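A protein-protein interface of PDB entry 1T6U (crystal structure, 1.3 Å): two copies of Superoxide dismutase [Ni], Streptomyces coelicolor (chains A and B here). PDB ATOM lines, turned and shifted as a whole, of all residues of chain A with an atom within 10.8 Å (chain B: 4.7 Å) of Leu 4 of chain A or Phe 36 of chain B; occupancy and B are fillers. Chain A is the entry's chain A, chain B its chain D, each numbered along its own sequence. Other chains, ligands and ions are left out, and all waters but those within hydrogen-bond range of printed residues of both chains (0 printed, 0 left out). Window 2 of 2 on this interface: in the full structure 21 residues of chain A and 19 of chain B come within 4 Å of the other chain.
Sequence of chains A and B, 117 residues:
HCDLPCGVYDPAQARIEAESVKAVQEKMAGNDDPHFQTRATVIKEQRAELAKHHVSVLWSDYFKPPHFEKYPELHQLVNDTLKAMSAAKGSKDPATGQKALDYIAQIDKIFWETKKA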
ATOM      1  N   HIS A   1      30.445  15.157  -3.675  1.00  0.00           N
ATOM      2  CA  HIS A   1      31.863  15.564  -3.663  1.00  0.00           C
ATOM      3  C   HIS A   1      32.509  14.996  -2.410  1.00  0.00           C
ATOM      4  O   HIS A   1      33.718  15.002  -2.186  1.00  0.00           O
ATOM      5  CB  HIS A   1      32.006  17.083  -3.669  1.00  0.00           C
ATOM      6  CG  HIS A   1      31.337  17.780  -2.517  1.00  0.00           C
ATOM      7  ND1 HIS A   1      30.465  17.080  -1.701  1.00  0.00           N
ATOM      8  CD2 HIS A   1      31.380  19.047  -2.026  1.00  0.00           C
ATOM      9  CE1 HIS A   1      30.012  17.908  -0.763  1.00  0.00           C
ATOM     10  NE2 HIS A   1      30.545  19.116  -0.943  1.00  0.00           N
ATOM     11  N   CYS A   2      31.602  14.547  -1.551  1.00  0.00           N
ATOM     12  CA  CYS A   2      31.959  14.082  -0.204  1.00  0.00           C
ATOM     13  C   CYS A   2      32.015  12.561  -0.073  1.00  0.00           C
ATOM     14  O   CYS A   2      32.260  12.096   1.033  1.00  0.00           O
ATOM     15  CB  CYS A   2      30.882  14.582   0.754  1.00  0.00           C
ATOM     16  SG  CYS A   2      29.257  14.284   0.058  1.00  0.00           S
ATOM     17  N   ASP A   3      31.737  11.830  -1.152  1.00  0.00           N
ATOM     18  CA  ASP A   3      31.851  10.368  -1.260  1.00  0.00           C
ATOM     19  C   ASP A   3      30.726   9.633  -0.535  1.00  0.00           C
ATOM     20  O   ASP A   3      30.849   8.430  -0.249  1.00  0.00           O
ATOM     21  CB  ASP A   3      33.215   9.930  -0.752  1.00  0.00           C
ATOM     22  CG  ASP A   3      33.914   8.828  -1.531  1.00  0.00           C
ATOM     23  OD1 ASP A   3      33.365   8.273  -2.493  1.00  0.00           O
ATOM     24  OD2 ASP A   3      35.087   8.567  -1.116  1.00  0.00           O
ATOM     25  N   LEU A   4      29.605  10.311  -0.281  1.00  0.00           N
ATOM     26  CA  LEU A   4      28.495   9.591   0.352  1.00  0.00           C
ATOM     27  C   LEU A   4      27.935   8.490  -0.519  1.00  0.00           C
ATOM     28  O   LEU A   4      27.766   7.345  -0.004  1.00  0.00           O
ATOM     29  CB  LEU A   4      27.368  10.547   0.801  1.00  0.00           C
ATOM     30  CG  LEU A   4      26.159   9.787   1.353  1.00  0.00           C
ATOM     31  CD1 LEU A   4      26.513   9.040   2.621  1.00  0.00           C
ATOM     32  CD2 LEU A   4      24.955  10.700   1.630  1.00  0.00           C
ATOM     33  N   PRO A   5      27.613   8.695  -1.788  1.00  0.00           N
ATOM     34  CA  PRO A   5      27.696   9.913  -2.578  1.00  0.00           C
ATOM     35  C   PRO A   5      26.570  10.913  -2.335  1.00  0.00           C
ATOM     36  O   PRO A   5      25.421  10.530  -2.078  1.00  0.00           O
ATOM     37  CB  PRO A   5      27.624   9.381  -4.027  1.00  0.00           C
ATOM     38  CG  PRO A   5      26.740   8.174  -3.899  1.00  0.00           C
ATOM     39  CD  PRO A   5      27.073   7.546  -2.561  1.00  0.00           C
ATOM     40  N   CYS A   6      26.905  12.221  -2.455  1.00  0.00           N
ATOM     41  CA  CYS A   6      25.880  13.256  -2.358  1.00  0.00           C
ATOM     42  C   CYS A   6      25.342  13.700  -3.699  1.00  0.00           C
ATOM     43  O   CYS A   6      24.288  14.319  -3.719  1.00  0.00           O
ATOM     44  CB  CYS A   6      26.416  14.476  -1.604  1.00  0.00           C
ATOM     45  SG  CYS A   6      27.674  15.391  -2.508  1.00  0.00           S
ATOM     46  N   GLY A   7      26.022  13.388  -4.781  1.00  0.00           N
ATOM     47  CA  GLY A   7      25.638  13.791  -6.121  1.00  0.00           C
ATOM     48  C   GLY A   7      25.921  15.234  -6.480  1.00  0.00           C
ATOM     49  O   GLY A   7      25.551  15.621  -7.591  1.00  0.00           O
ATOM     50  N   VAL A   8      26.570  15.994  -5.611  1.00  0.00           N
ATOM     51  CA  VAL A   8      26.901  17.397  -5.853  1.00  0.00           C
ATOM     52  C   VAL A   8      28.373  17.534  -6.255  1.00  0.00           C
ATOM     53  O   VAL A   8      29.256  17.186  -5.491  1.00  0.00           O
ATOM     54  CB  VAL A   8      26.616  18.270  -4.618  1.00  0.00           C
ATOM     55  CG1 VAL A   8      26.983  19.732  -4.848  1.00  0.00           C
ATOM     56  CG2 VAL A   8      25.147  18.195  -4.263  1.00  0.00           C
ATOM     57  N   TYR A   9      28.579  18.035  -7.457  1.00  0.00           N
ATOM     58  CA  TYR A   9      29.924  18.335  -7.942  1.00  0.00           C
ATOM     59  C   TYR A   9      29.952  19.595  -8.770  1.00  0.00           C
ATOM     60  O   TYR A   9      28.995  19.908  -9.469  1.00  0.00           O
ATOM     61  CB  TYR A   9      30.490  17.245  -8.873  1.00  0.00           C
ATOM     62  CG  TYR A   9      30.563  15.871  -8.257  1.00  0.00           C
ATOM     63  CD1 TYR A   9      29.474  15.034  -8.296  1.00  0.00           C
ATOM     64  CD2 TYR A   9      31.715  15.455  -7.632  1.00  0.00           C
ATOM     65  CE1 TYR A   9      29.573  13.785  -7.718  1.00  0.00           C
ATOM     66  CE2 TYR A   9      31.823  14.217  -7.061  1.00  0.00           C
ATOM     67  CZ  TYR A   9      30.729  13.394  -7.111  1.00  0.00           C
ATOM     68  OH  TYR A   9      30.798  12.140  -6.552  1.00  0.00           O
ATOM     69  N   VAL A  57      39.070  14.328  -6.718  1.00  0.00           N
ATOM     70  CA  VAL A  57      37.718  13.869  -6.437  1.00  0.00           C
ATOM     71  C   VAL A  57      36.857  13.852  -7.692  1.00  0.00           C
ATOM     72  O   VAL A  57      36.085  12.921  -7.927  1.00  0.00           O
ATOM     73  CB  VAL A  57      37.122  14.777  -5.331  1.00  0.00           C
ATOM     74  CG1 VAL A  57      35.608  14.659  -5.285  1.00  0.00           C
ATOM     75  CG2 VAL A  57      37.732  14.454  -3.957  1.00  0.00           C
ATOM     76  N   SER A  60      38.068  10.659  -9.528  1.00  0.00           N
ATOM     77  CA  SER A  60      37.773   9.347  -8.949  1.00  0.00           C
ATOM     78  C   SER A  60      36.299   9.134  -8.668  1.00  0.00           C
ATOM     79  O   SER A  60      35.761   8.034  -8.720  1.00  0.00           O
ATOM     80  CB  SER A  60      38.522   9.110  -7.632  1.00  0.00           C
ATOM     81  OG  SER A  60      38.174  10.097  -6.648  1.00  0.00           O
ATOM     82  N   ASP A  61      35.592  10.204  -8.304  1.00  0.00           N
ATOM     83  CA  ASP A  61      34.243  10.029  -7.764  1.00  0.00           C
ATOM     84  C   ASP A  61      33.153  10.453  -8.734  1.00  0.00           C
ATOM     85  O   ASP A  61      32.146   9.769  -8.780  1.00  0.00           O
ATOM     86  CB  ASP A  61      34.136  10.827  -6.460  1.00  0.00           C
ATOM     87  CG  ASP A  61      35.002  10.343  -5.312  1.00  0.00           C
ATOM     88  OD1 ASP A  61      35.865   9.472  -5.468  1.00  0.00           O
ATOM     89  OD2 ASP A  61      34.816  10.883  -4.188  1.00  0.00           O
ATOM     90  N   TYR A  62      33.340  11.528  -9.470  1.00  0.00           N
ATOM     91  CA  TYR A  62      32.325  11.942 -10.455  1.00  0.00           C
ATOM     92  C   TYR A  62      32.454  11.166 -11.740  1.00  0.00           C
ATOM     93  O   TYR A  62      31.493  10.538 -12.254  1.00  0.00           O
ATOM     94  CB  TYR A  62      32.391  13.471 -10.726  1.00  0.00           C
ATOM     95  CG  TYR A  62      31.417  13.745 -11.868  1.00  0.00           C
ATOM     96  CD1 TYR A  62      30.058  13.850 -11.646  1.00  0.00           C
ATOM     97  CD2 TYR A  62      31.865  13.904 -13.161  1.00  0.00           C
ATOM     98  CE1 TYR A  62      29.156  14.094 -12.667  1.00  0.00           C
ATOM     99  CE2 TYR A  62      30.968  14.133 -14.205  1.00  0.00           C
ATOM    100  CZ  TYR A  62      29.609  14.237 -13.960  1.00  0.00           C
ATOM    101  OH  TYR A  62      28.695  14.475 -14.961  1.00  0.00           O
ATOM    102  N   LYS A  64      33.136   8.405 -14.563  1.00  0.00           N
ATOM    103  CA  LYS A  64      32.890   6.969 -14.580  1.00  0.00           C
ATOM    104  C   LYS A  64      33.308   6.363 -15.917  1.00  0.00           C
ATOM    105  O   LYS A  64      33.627   7.053 -16.866  1.00  0.00           O
ATOM    106  CB  LYS A  64      31.441   6.615 -14.396  1.00  0.00           C
ATOM    107  CG  LYS A  64      30.705   7.324 -13.304  1.00  0.00           C
ATOM    108  CD  LYS A  64      30.649   6.571 -12.005  1.00  0.00           C
ATOM    109  CE  LYS A  64      30.280   7.479 -10.832  1.00  0.00           C
ATOM    110  NZ  LYS A  64      29.313   6.846  -9.894  1.00  0.00           N
ATOM    111  N   VAL B  24      22.340  15.548   1.029  1.00  0.00           N
ATOM    112  CA  VAL B  24      22.501  14.467   2.004  1.00  0.00           C
ATOM    113  C   VAL B  24      21.205  14.232   2.747  1.00  0.00           C
ATOM    114  O   VAL B  24      20.782  13.081   2.887  1.00  0.00           O
ATOM    115  CB  VAL B  24      23.684  14.742   2.933  1.00  0.00           C
ATOM    116  CG1 VAL B  24      23.731  13.702   4.042  1.00  0.00           C
ATOM    117  CG2 VAL B  24      24.961  14.699   2.111  1.00  0.00           C
ATOM    118  N   LYS B  27      18.926  12.384   0.655  1.00  0.00           N
ATOM    119  CA  LYS B  27      19.296  10.957   0.547  1.00  0.00           C
ATOM    120  C   LYS B  27      18.926  10.142   1.766  1.00  0.00           C
ATOM    121  O   LYS B  27      18.633   8.922   1.693  1.00  0.00           O
ATOM    122  CB  LYS B  27      20.806  10.839   0.266  1.00  0.00           C
ATOM    123  CG  LYS B  27      21.229  11.460  -1.059  1.00  0.00           C
ATOM    124  CD  LYS B  27      21.692  10.544  -2.133  1.00  0.00           C
ATOM    125  CE  LYS B  27      22.327  11.260  -3.330  1.00  0.00           C
ATOM    126  NZ  LYS B  27      21.573  10.976  -4.586  1.00  0.00           N
ATOM    127  N   MET B  28      18.948  10.791   2.926  1.00  0.00           N
ATOM    128  CA  MET B  28      18.633  10.040   4.145  1.00  0.00           C
ATOM    129  C   MET B  28      17.176   9.561   4.156  1.00  0.00           C
ATOM    130  O   MET B  28      16.902   8.631   4.891  1.00  0.00           O
ATOM    131  CB  MET B  28      18.923  10.892   5.378  1.00  0.00           C
ATOM    132  CG  MET B  28      20.401  11.189   5.541  1.00  0.00           C
ATOM    133  SD  MET B  28      20.852  12.196   6.976  1.00  0.00           S
ATOM    134  CE  MET B  28      20.906  10.928   8.229  1.00  0.00           C
ATOM    135  N   ASN B  31      16.870   5.542   2.347  1.00  0.00           N
ATOM    136  CA  ASN B  31      17.603   4.340   2.709  1.00  0.00           C
ATOM    137  C   ASN B  31      17.829   4.325   4.217  1.00  0.00           C
ATOM    138  O   ASN B  31      18.738   5.041   4.614  1.00  0.00           O
ATOM    139  CB  ASN B  31      18.976   4.344   2.054  1.00  0.00           C
ATOM    140  CG  ASN B  31      19.828   3.150   2.345  1.00  0.00           C
ATOM    141  OD1 ASN B  31      19.482   2.268   3.120  1.00  0.00           O
ATOM    142  ND2 ASN B  31      20.973   3.078   1.690  1.00  0.00           N
ATOM    143  N   ASP B  33      19.043   2.021   6.034  1.00  0.00           N
ATOM    144  CA  ASP B  33      20.173   1.243   6.577  1.00  0.00           C
ATOM    145  C   ASP B  33      20.924   2.017   7.624  1.00  0.00           C
ATOM    146  O   ASP B  33      21.342   3.159   7.362  1.00  0.00           O
ATOM    147  CB  ASP B  33      21.139   0.861   5.467  1.00  0.00           C
ATOM    148  CG  ASP B  33      22.308   0.055   5.998  1.00  0.00           C
ATOM    149  OD1 ASP B  33      22.082  -1.014   6.607  1.00  0.00           O
ATOM    150  OD2 ASP B  33      23.460   0.503   5.835  1.00  0.00           O
ATOM    151  N   PRO B  34      21.135   1.512   8.818  1.00  0.00           N
ATOM    152  CA  PRO B  34      21.887   2.302   9.831  1.00  0.00           C
ATOM    153  C   PRO B  34      23.261   2.770   9.402  1.00  0.00           C
ATOM    154  O   PRO B  34      23.677   3.898   9.647  1.00  0.00           O
ATOM    155  CB  PRO B  34      21.978   1.285  10.965  1.00  0.00           C
ATOM    156  CG  PRO B  34      20.657   0.559  10.812  1.00  0.00           C
ATOM    157  CD  PRO B  34      20.628   0.229   9.320  1.00  0.00           C
ATOM    158  N   HIS B  35      24.018   1.892   8.730  1.00  0.00           N
ATOM    159  CA  HIS B  35      25.383   2.251   8.308  1.00  0.00           C
ATOM    160  C   HIS B  35      25.311   3.470   7.384  1.00  0.00           C
ATOM    161  O   HIS B  35      26.054   4.441   7.513  1.00  0.00           O
ATOM    162  CB  HIS B  35      26.090   1.055   7.676  1.00  0.00           C
ATOM    163  CG  HIS B  35      27.508   1.230   7.262  1.00  0.00           C
ATOM    164  ND1 HIS B  35      28.520   1.425   8.182  1.00  0.00           N
ATOM    165  CD2 HIS B  35      28.118   1.244   6.050  1.00  0.00           C
ATOM    166  CE1 HIS B  35      29.666   1.544   7.534  1.00  0.00           C
ATOM    167  NE2 HIS B  35      29.493   1.447   6.262  1.00  0.00           N
ATOM    168  N   PHE B  36      24.386   3.432   6.418  1.00  0.00           N
ATOM    169  CA  PHE B  36      24.240   4.565   5.508  1.00  0.00           C
ATOM    170  C   PHE B  36      23.808   5.808   6.266  1.00  0.00           C
ATOM    171  O   PHE B  36      24.337   6.916   6.039  1.00  0.00           O
ATOM    172  CB  PHE B  36      23.218   4.196   4.418  1.00  0.00           C
ATOM    173  CG  PHE B  36      23.050   5.378   3.459  1.00  0.00           C
ATOM    174  CD1 PHE B  36      21.929   6.177   3.553  1.00  0.00           C
ATOM    175  CD2 PHE B  36      24.032   5.615   2.511  1.00  0.00           C
ATOM    176  CE1 PHE B  36      21.794   7.268   2.667  1.00  0.00           C
ATOM    177  CE2 PHE B  36      23.898   6.700   1.664  1.00  0.00           C
ATOM    178  CZ  PHE B  36      22.786   7.521   1.737  1.00  0.00           C
ATOM    179  N   GLN B  37      22.833   5.644   7.149  1.00  0.00           N
ATOM    180  CA  GLN B  37      22.364   6.778   7.921  1.00  0.00           C
ATOM    181  C   GLN B  37      23.532   7.417   8.656  1.00  0.00           C
ATOM    182  O   GLN B  37      23.647   8.652   8.756  1.00  0.00           O
ATOM    183  CB  GLN B  37      21.299   6.401   8.941  1.00  0.00           C
ATOM    184  CG  GLN B  37      19.959   6.040   8.312  1.00  0.00           C
ATOM    185  CD  GLN B  37      19.162   7.224   7.830  1.00  0.00           C
ATOM    186  OE1 GLN B  37      18.958   8.191   8.579  1.00  0.00           O
ATOM    187  NE2 GLN B  37      18.699   7.131   6.561  1.00  0.00           N
ATOM    188  N   THR B  38      24.412   6.595   9.202  1.00  0.00           N
ATOM    189  CA  THR B  38      25.556   7.080   9.988  1.00  0.00           C
ATOM    190  C   THR B  38      26.547   7.789   9.084  1.00  0.00           C
ATOM    191  O   THR B  38      27.061   8.871   9.444  1.00  0.00           O
ATOM    192  CB  THR B  38      26.210   5.962  10.810  1.00  0.00           C
ATOM    193  OG1 THR B  38      25.281   5.530  11.812  1.00  0.00           O
ATOM    194  CG2 THR B  38      27.448   6.479  11.544  1.00  0.00           C
ATOM    195  N   ARG B  39      26.853   7.234   7.911  1.00  0.00           N
ATOM    196  CA  ARG B  39      27.796   7.897   7.002  1.00  0.00           C
ATOM    197  C   ARG B  39      27.229   9.240   6.549  1.00  0.00           C
ATOM    198  O   ARG B  39      27.974  10.228   6.478  1.00  0.00           O
ATOM    199  CB  ARG B  39      28.117   7.002   5.808  1.00  0.00           C
ATOM    200  CG  ARG B  39      28.882   5.726   6.164  1.00  0.00           C
ATOM    201  CD  ARG B  39      29.213   4.900   4.929  1.00  0.00           C
ATOM    202  NE  ARG B  39      29.981   5.755   4.029  1.00  0.00           N
ATOM    203  CZ  ARG B  39      29.680   6.206   2.815  1.00  0.00           C
ATOM    204  NH1 ARG B  39      28.535   5.850   2.217  1.00  0.00           N
ATOM    205  NH2 ARG B  39      30.486   7.022   2.127  1.00  0.00           N
ATOM    206  N   ALA B  40      25.924   9.233   6.259  1.00  0.00           N
ATOM    207  CA  ALA B  40      25.291  10.476   5.864  1.00  0.00           C
ATOM    208  C   ALA B  40      25.394  11.531   6.958  1.00  0.00           C
ATOM    209  O   ALA B  40      25.638  12.728   6.741  1.00  0.00           O
ATOM    210  CB  ALA B  40      23.839  10.193   5.500  1.00  0.00           C
ATOM    211  N   ILE B  43      29.022  12.870   7.165  1.00  0.00           N
ATOM    212  CA  ILE B  43      29.349  13.722   6.055  1.00  0.00           C
ATOM    213  C   ILE B  43      28.580  15.035   6.072  1.00  0.00           C
ATOM    214  O   ILE B  43      29.154  16.101   5.795  1.00  0.00           O
ATOM    215  CB  ILE B  43      29.118  12.934   4.751  1.00  0.00           C
ATOM    216  CG1 ILE B  43      30.244  11.908   4.583  1.00  0.00           C
ATOM    217  CG2 ILE B  43      28.973  13.875   3.576  1.00  0.00           C
ATOM    218  CD1 ILE B  43      29.891  10.822   3.565  1.00  0.00           C
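O of Leu 4 of chain A lies within hydrogen-bond range of NH1 of Arg 39 of chain B (2.8 Å). NH2 of Arg 39 of chain B lies within hydrogen-bond range of O of Asp 3 of chain A (2.8 Å).
The side-chain carboxylate of Asp 33 of chain B sits at hydrogen-bond distance from the backbone NH of Phe 36 of chain B (3.1 Å). The backbone NH of Val 8 of chain A sits close to the side-chain sulfur of Cys 6 of chain A.
CB of Cys 2 of chain A touches CG2 of Ile 43 of chain B, at 3.5 Å. Leu 4 of chain A touches Phe 36 of chain B (CD1 to CE2, 3.6 Å). Ala 40 of chain B touches Leu 4 of chain A. Ile 43 of chain B touches Leu 4 of chain A (CD1 to CA, 3.7 Å). Lys 27 of chain B touches Pro 5 of chain A (CE to O, 3.4 Å). Cys 6 of chain A touches Val 24 of chain B. CE of Lys 27 of chain B touches O of Cys 6 of chain A (3.7 Å).
Printed residues of chain B within 4 Å of Cys 2 of chain A: Ile 43. Of the printed residues of chain B, Asp 3 of chain A touches Arg 39. Met 28 of chain B touches none of the printed residues of chain A. No residue of chain A comes within 4 Å of Asn 31 of chain B. No residue of chain A comes within 4 Å of Pro 34 of chain B. Printed residues of chain A within 4 Å of Phe 36 of chain B: Leu 4. No residue of chain A comes within 4 Å of Gln 37 of chain B. No residue of chain A comes within 4 Å of Thr 38 of chain B. Arg 39 of chain B touches just these residues of chain A: Asp 3 and Leu 4. Ala 40 of chain B touches just one residue of chain A: Leu 4. The nearest printed residue of chain B that does not touch Pro 5 of chain A is Arg 39 of chain B (5.0 Å).
Of the 14 printed residues of chain A, 5 touch a printed residue of chain B. Hydrophobic or aromatic side chains of chain A within 4 Å of the printed part of chain B: Leu 4. Along chain A the printed residues that touch a printed residue of chain B span positions 2 to 6. Hydrophobic or aromatic side chains of chain B that line the printed part of chain A: Val 24, Phe 36 and Ile 43. Among the printed residues, 9 pairs touch across the chains.
No position is printed for both chains. Of the 9 pairs that touch across the chains among the printed residues, none has its exchanged pair printed and touching as well.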
